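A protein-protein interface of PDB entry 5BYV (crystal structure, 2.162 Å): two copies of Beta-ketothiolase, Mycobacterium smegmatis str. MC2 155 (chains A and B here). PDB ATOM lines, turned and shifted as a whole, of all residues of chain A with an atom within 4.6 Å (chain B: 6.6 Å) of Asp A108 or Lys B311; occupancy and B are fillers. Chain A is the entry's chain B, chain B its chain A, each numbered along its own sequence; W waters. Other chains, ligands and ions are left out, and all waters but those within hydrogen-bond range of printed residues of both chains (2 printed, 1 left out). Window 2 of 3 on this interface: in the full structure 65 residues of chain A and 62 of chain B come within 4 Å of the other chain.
Of chain A, only Asp A108 (2.9 Å) comes within 4 Å of Lys B311.
Printed residues of chain A within 4 Å of Leu B102: Gln A103 (3.7 Å), Ser A106 (3.95 Å) and Asp A108 (3.8 Å).
Of the printed residues of chain B, Gln A103 touches Leu B102.
Ala B312 touches none of the printed residues of chain A.
Glu A51 touches none of the printed residues of chain B.
The nearest printed residue of chain A that does not touch Lys B311 is Gly A107 (5.1 Å).
Water W1 lies within hydrogen-bond range of the backbone carbonyl oxygen (O) of Glu A51 (2.7 Å) and the backbone carbonyl oxygen (O) of Ser B289 (3.5 Å).
Water W2 lies within hydrogen-bond range of a ring nitrogen (NE2) of His A109 (3.1 Å) and the backbone NH (N) of Ser B289 (3.2 Å).
No position is printed for both chains.
The indole nitrogen (NE1) of Trp B287 lies within hydrogen-bond range of the side-chain carboxylate (OD2) of Asp A108 (3.3 Å).
The side-chain amino group of Lys B311 is in salt-bridge range of the side-chain carboxylate of Asp A108 (2.9 Å).
Of the 7 printed residues of chain A, 4 touch a printed residue of chain B.
Printed residues of chain B that touch a printed residue of chain A: Leu B102, Trp B287, Ser B289 and Lys B311.
Along chain B the printed residues that touch a printed residue of chain A span positions 102 to 311.
Among the printed residues, Asp or Glu carboxylates within 4 Å of a Lys or Arg side-chain nitrogen of the other chain: Asp A108 with Lys B311 (2.9 Å).
CD1 of Leu B102 touches CB of Gln A103, 3.7 Å away.
CD2 of Leu B102 touches OG of Ser A106, 3.95 Å away.
CD2 of Leu B102 touches OD2 of Asp A108, at 3.8 Å.
Trp B287 touches His A109 (CH2 to CE1, 3.6 Å).
Ser B289 touches His A109.
O of Trp B287 sits at hydrogen-bond distance from NZ of Lys B311 (2.4 Å).
NE2 of Gln A103 lies within hydrogen-bond range of ND1 of His A109 (2.8 Å).
OG of Ser A106 sits at hydrogen-bond distance from OD2 of Asp A108 (2.4 Å).
OG of Ser A106 is in hydrogen-bond range of O of Gln A103.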
ATOM      1  N   GLU A  51      37.151   9.479  16.682  1.00  0.00           N
ATOM      2  CA  GLU A  51      35.805  10.061  16.805  1.00  0.00           C
ATOM      3  C   GLU A  51      35.609  10.996  18.005  1.00  0.00           C
ATOM      4  O   GLU A  51      34.568  11.631  18.148  1.00  0.00           O
ATOM      5  CB  GLU A  51      34.764   8.935  16.876  1.00  0.00           C
ATOM      6  CG  GLU A  51      34.694   8.057  15.632  1.00  0.00           C
ATOM      7  CD  GLU A  51      33.813   6.837  15.822  1.00  0.00           C
ATOM      8  OE1 GLU A  51      32.583   7.009  15.740  1.00  0.00           O
ATOM      9  OE2 GLU A  51      34.345   5.715  16.004  1.00  0.00           O
ATOM     10  N   GLN A 103      31.765   4.711  25.857  1.00  0.00           N
ATOM     11  CA  GLN A 103      31.164   5.163  24.618  1.00  0.00           C
ATOM     12  C   GLN A 103      31.681   4.374  23.421  1.00  0.00           C
ATOM     13  O   GLN A 103      31.200   4.534  22.303  1.00  0.00           O
ATOM     14  CB  GLN A 103      31.380   6.678  24.434  1.00  0.00           C
ATOM     15  CG  GLN A 103      32.763   7.154  24.026  1.00  0.00           C
ATOM     16  CD  GLN A 103      32.868   8.688  24.051  1.00  0.00           C
ATOM     17  OE1 GLN A 103      32.630   9.319  25.080  1.00  0.00           O
ATOM     18  NE2 GLN A 103      33.226   9.282  22.919  1.00  0.00           N
ATOM     19  N   SER A 106      29.541   0.818  23.943  1.00  0.00           N
ATOM     20  CA  SER A 106      28.129   1.005  23.694  1.00  0.00           C
ATOM     21  C   SER A 106      27.752   0.975  22.214  1.00  0.00           C
ATOM     22  O   SER A 106      26.564   0.982  21.891  1.00  0.00           O
ATOM     23  CB  SER A 106      27.679   2.340  24.277  1.00  0.00           C
ATOM     24  OG  SER A 106      28.140   3.398  23.451  1.00  0.00           O
ATOM     25  N   GLY A 107      28.737   1.010  21.320  1.00  0.00           N
ATOM     26  CA  GLY A 107      28.462   1.039  19.893  1.00  0.00           C
ATOM     27  C   GLY A 107      28.413   2.430  19.293  1.00  0.00           C
ATOM     28  O   GLY A 107      28.346   2.608  18.068  1.00  0.00           O
ATOM     29  N   ASP A 108      28.453   3.433  20.161  1.00  0.00           N
ATOM     30  CA  ASP A 108      28.381   4.827  19.728  1.00  0.00           C
ATOM     31  C   ASP A 108      29.606   5.221  18.912  1.00  0.00           C
ATOM     32  O   ASP A 108      29.497   5.886  17.885  1.00  0.00           O
ATOM     33  CB  ASP A 108      28.243   5.738  20.945  1.00  0.00           C
ATOM     34  CG  ASP A 108      26.888   5.632  21.595  1.00  0.00           C
ATOM     35  OD1 ASP A 108      25.888   5.866  20.887  1.00  0.00           O
ATOM     36  OD2 ASP A 108      26.821   5.315  22.803  1.00  0.00           O
ATOM     37  N   HIS A 109      30.767   4.780  19.384  1.00  0.00           N
ATOM     38  CA  HIS A 109      32.039   5.043  18.730  1.00  0.00           C
ATOM     39  C   HIS A 109      32.828   3.753  18.603  1.00  0.00           C
ATOM     40  O   HIS A 109      32.683   2.839  19.418  1.00  0.00           O
ATOM     41  CB  HIS A 109      32.849   6.080  19.520  1.00  0.00           C
ATOM     42  CG  HIS A 109      32.338   7.480  19.393  1.00  0.00           C
ATOM     43  ND1 HIS A 109      32.554   8.437  20.361  1.00  0.00           N
ATOM     44  CD2 HIS A 109      31.662   8.100  18.397  1.00  0.00           C
ATOM     45  CE1 HIS A 109      32.015   9.580  19.976  1.00  0.00           C
ATOM     46  NE2 HIS A 109      31.463   9.402  18.788  1.00  0.00           N
ATOM     47  N   ASP A 110      33.670   3.672  17.586  1.00  0.00           N
ATOM     48  CA  ASP A 110      34.513   2.505  17.431  1.00  0.00           C
ATOM     49  C   ASP A 110      35.912   2.808  17.939  1.00  0.00           C
ATOM     50  O   ASP A 110      36.613   1.925  18.430  1.00  0.00           O
ATOM     51  CB  ASP A 110      34.562   2.056  15.965  1.00  0.00           C
ATOM     52  CG  ASP A 110      33.248   1.483  15.483  1.00  0.00           C
ATOM     53  OD1 ASP A 110      32.475   0.992  16.330  1.00  0.00           O
ATOM     54  OD2 ASP A 110      32.995   1.514  14.259  1.00  0.00           O
ATOM     55  N   ILE B  98      24.459  12.459  28.659  1.00  0.00           N
ATOM     56  CA  ILE B  98      24.901  11.320  27.865  1.00  0.00           C
ATOM     57  C   ILE B  98      25.885  10.451  28.644  1.00  0.00           C
ATOM     58  O   ILE B  98      25.780   9.233  28.615  1.00  0.00           O
ATOM     59  CB  ILE B  98      25.521  11.783  26.526  1.00  0.00           C
ATOM     60  CG1 ILE B  98      24.421  12.329  25.616  1.00  0.00           C
ATOM     61  CG2 ILE B  98      26.255  10.648  25.847  1.00  0.00           C
ATOM     62  CD1 ILE B  98      24.925  13.168  24.484  1.00  0.00           C
ATOM     63  N   LEU B 102      25.306   6.519  29.819  1.00  0.00           N
ATOM     64  CA  LEU B 102      26.248   5.462  29.514  1.00  0.00           C
ATOM     65  C   LEU B 102      26.560   4.621  30.742  1.00  0.00           C
ATOM     66  O   LEU B 102      26.570   3.396  30.661  1.00  0.00           O
ATOM     67  CB  LEU B 102      27.525   6.041  28.916  1.00  0.00           C
ATOM     68  CG  LEU B 102      27.370   6.580  27.485  1.00  0.00           C
ATOM     69  CD1 LEU B 102      28.683   7.148  26.968  1.00  0.00           C
ATOM     70  CD2 LEU B 102      26.879   5.483  26.560  1.00  0.00           C
ATOM     71  N   VAL B 285      17.430   7.518  23.191  1.00  0.00           N
ATOM     72  CA  VAL B 285      17.479   6.618  22.046  1.00  0.00           C
ATOM     73  C   VAL B 285      18.892   6.532  21.492  1.00  0.00           C
ATOM     74  O   VAL B 285      19.483   5.447  21.421  1.00  0.00           O
ATOM     75  CB  VAL B 285      16.523   7.076  20.928  1.00  0.00           C
ATOM     76  CG1 VAL B 285      16.482   6.057  19.794  1.00  0.00           C
ATOM     77  CG2 VAL B 285      15.138   7.308  21.487  1.00  0.00           C
ATOM     78  N   SER B 286      19.419   7.696  21.118  1.00  0.00           N
ATOM     79  CA  SER B 286      20.714   7.810  20.454  1.00  0.00           C
ATOM     80  C   SER B 286      21.307   9.203  20.653  1.00  0.00           C
ATOM     81  O   SER B 286      20.615  10.119  21.094  1.00  0.00           O
ATOM     82  CB  SER B 286      20.567   7.524  18.964  1.00  0.00           C
ATOM     83  OG  SER B 286      19.953   8.634  18.338  1.00  0.00           O
ATOM     84  N   TRP B 287      22.582   9.360  20.322  1.00  0.00           N
ATOM     85  CA  TRP B 287      23.217  10.674  20.342  1.00  0.00           C
ATOM     86  C   TRP B 287      24.334  10.721  19.322  1.00  0.00           C
ATOM     87  O   TRP B 287      24.874   9.686  18.942  1.00  0.00           O
ATOM     88  CB  TRP B 287      23.768  11.011  21.730  1.00  0.00           C
ATOM     89  CG  TRP B 287      24.800  10.073  22.243  1.00  0.00           C
ATOM     90  CD1 TRP B 287      24.597   9.013  23.068  1.00  0.00           C
ATOM     91  CD2 TRP B 287      26.208  10.115  21.984  1.00  0.00           C
ATOM     92  NE1 TRP B 287      25.791   8.387  23.344  1.00  0.00           N
ATOM     93  CE2 TRP B 287      26.796   9.048  22.688  1.00  0.00           C
ATOM     94  CE3 TRP B 287      27.029  10.949  21.218  1.00  0.00           C
ATOM     95  CZ2 TRP B 287      28.177   8.790  22.648  1.00  0.00           C
ATOM     96  CZ3 TRP B 287      28.396  10.692  21.177  1.00  0.00           C
ATOM     97  CH2 TRP B 287      28.956   9.627  21.885  1.00  0.00           C
ATOM     98  N   GLY B 288      24.697  11.917  18.888  1.00  0.00           N
ATOM     99  CA  GLY B 288      25.836  12.046  18.004  1.00  0.00           C
ATOM    100  C   GLY B 288      26.637  13.295  18.279  1.00  0.00           C
ATOM    101  O   GLY B 288      26.091  14.319  18.704  1.00  0.00           O
ATOM    102  N   SER B 289      27.938  13.210  18.030  1.00  0.00           N
ATOM    103  CA  SER B 289      28.809  14.376  18.091  1.00  0.00           C
ATOM    104  C   SER B 289      29.522  14.585  16.758  1.00  0.00           C
ATOM    105  O   SER B 289      29.715  13.645  15.992  1.00  0.00           O
ATOM    106  CB  SER B 289      29.817  14.226  19.214  1.00  0.00           C
ATOM    107  OG  SER B 289      30.775  13.249  18.899  1.00  0.00           O
ATOM    108  N   GLU B 306      22.447  14.361  12.126  1.00  0.00           N
ATOM    109  CA  GLU B 306      22.428  13.239  11.205  1.00  0.00           C
ATOM    110  C   GLU B 306      23.013  11.999  11.856  1.00  0.00           C
ATOM    111  O   GLU B 306      22.473  10.907  11.705  1.00  0.00           O
ATOM    112  CB  GLU B 306      23.183  13.574   9.926  1.00  0.00           C
ATOM    113  CG  GLU B 306      22.331  14.350   8.924  1.00  0.00           C
ATOM    114  CD  GLU B 306      22.849  14.194   7.520  1.00  0.00           C
ATOM    115  OE1 GLU B 306      23.751  13.342   7.330  1.00  0.00           O
ATOM    116  OE2 GLU B 306      22.355  14.905   6.613  1.00  0.00           O
ATOM    117  N   VAL B 307      24.104  12.161  12.593  1.00  0.00           N
ATOM    118  CA  VAL B 307      24.709  11.011  13.244  1.00  0.00           C
ATOM    119  C   VAL B 307      23.680  10.400  14.182  1.00  0.00           C
ATOM    120  O   VAL B 307      23.446   9.199  14.152  1.00  0.00           O
ATOM    121  CB  VAL B 307      26.006  11.385  14.008  1.00  0.00           C
ATOM    122  CG1 VAL B 307      26.498  10.215  14.850  1.00  0.00           C
ATOM    123  CG2 VAL B 307      27.078  11.825  13.029  1.00  0.00           C
ATOM    124  N   ALA B 308      23.018  11.237  14.966  1.00  0.00           N
ATOM    125  CA  ALA B 308      22.120  10.746  15.993  1.00  0.00           C
ATOM    126  C   ALA B 308      20.875  10.119  15.379  1.00  0.00           C
ATOM    127  O   ALA B 308      20.419   9.075  15.843  1.00  0.00           O
ATOM    128  CB  ALA B 308      21.744  11.856  16.936  1.00  0.00           C
ATOM    129  N   LEU B 309      20.321  10.752  14.346  1.00  0.00           N
ATOM    130  CA  LEU B 309      19.164  10.195  13.652  1.00  0.00           C
ATOM    131  C   LEU B 309      19.526   8.860  13.020  1.00  0.00           C
ATOM    132  O   LEU B 309      18.737   7.922  13.042  1.00  0.00           O
ATOM    133  CB  LEU B 309      18.641  11.159  12.581  1.00  0.00           C
ATOM    134  CG  LEU B 309      18.030  12.481  13.046  1.00  0.00           C
ATOM    135  CD1 LEU B 309      17.689  13.368  11.871  1.00  0.00           C
ATOM    136  CD2 LEU B 309      16.805  12.207  13.878  1.00  0.00           C
ATOM    137  N   ALA B 310      20.734   8.777  12.473  1.00  0.00           N
ATOM    138  CA  ALA B 310      21.202   7.559  11.827  1.00  0.00           C
ATOM    139  C   ALA B 310      21.293   6.381  12.799  1.00  0.00           C
ATOM    140  O   ALA B 310      20.835   5.279  12.499  1.00  0.00           O
ATOM    141  CB  ALA B 310      22.552   7.801  11.171  1.00  0.00           C
ATOM    142  N   LYS B 311      21.888   6.611  13.963  1.00  0.00           N
ATOM    143  CA  LYS B 311      22.038   5.556  14.951  1.00  0.00           C
ATOM    144  C   LYS B 311      20.686   5.170  15.542  1.00  0.00           C
ATOM    145  O   LYS B 311      20.531   4.083  16.091  1.00  0.00           O
ATOM    146  CB  LYS B 311      23.011   6.003  16.049  1.00  0.00           C
ATOM    147  CG  LYS B 311      24.302   6.580  15.489  1.00  0.00           C
ATOM    148  CD  LYS B 311      25.465   6.501  16.450  1.00  0.00           C
ATOM    149  CE  LYS B 311      25.061   6.902  17.852  1.00  0.00           C
ATOM    150  NZ  LYS B 311      26.133   7.620  18.608  1.00  0.00           N
ATOM    151  N   ALA B 312      19.704   6.056  15.408  1.00  0.00           N
ATOM    152  CA  ALA B 312      18.357   5.786  15.905  1.00  0.00           C
ATOM    153  C   ALA B 312      17.469   5.178  14.829  1.00  0.00           C
ATOM    154  O   ALA B 312      16.308   4.863  15.085  1.00  0.00           O
ATOM    155  CB  ALA B 312      17.726   7.058  16.426  1.00  0.00           C
ATOM    156  N   GLY B 313      18.015   5.033  13.625  1.00  0.00           N
ATOM    157  CA  GLY B 313      17.241   4.573  12.489  1.00  0.00           C
ATOM    158  C   GLY B 313      16.057   5.482  12.196  1.00  0.00           C
ATOM    159  O   GLY B 313      15.017   5.019  11.722  1.00  0.00           O
ATOM    160  N   LEU B 314      16.204   6.771  12.488  1.00  0.00           N
ATOM    161  CA  LEU B 314      15.134   7.736  12.249  1.00  0.00           C
ATOM    162  C   LEU B 314      15.523   8.741  11.175  1.00  0.00           C
ATOM    163  O   LEU B 314      16.677   8.792  10.744  1.00  0.00           O
ATOM    164  CB  LEU B 314      14.779   8.477  13.538  1.00  0.00           C
ATOM    165  CG  LEU B 314      14.290   7.653  14.727  1.00  0.00           C
ATOM    166  CD1 LEU B 314      14.000   8.548  15.921  1.00  0.00           C
ATOM    167  CD2 LEU B 314      13.054   6.860  14.342  1.00  0.00           C
HETATM  168  O   HOH W   1      32.598  11.701  16.316  1.00  0.00           O
HETATM  169  O   HOH W   2      28.749  10.142  17.595  1.00  0.00           O
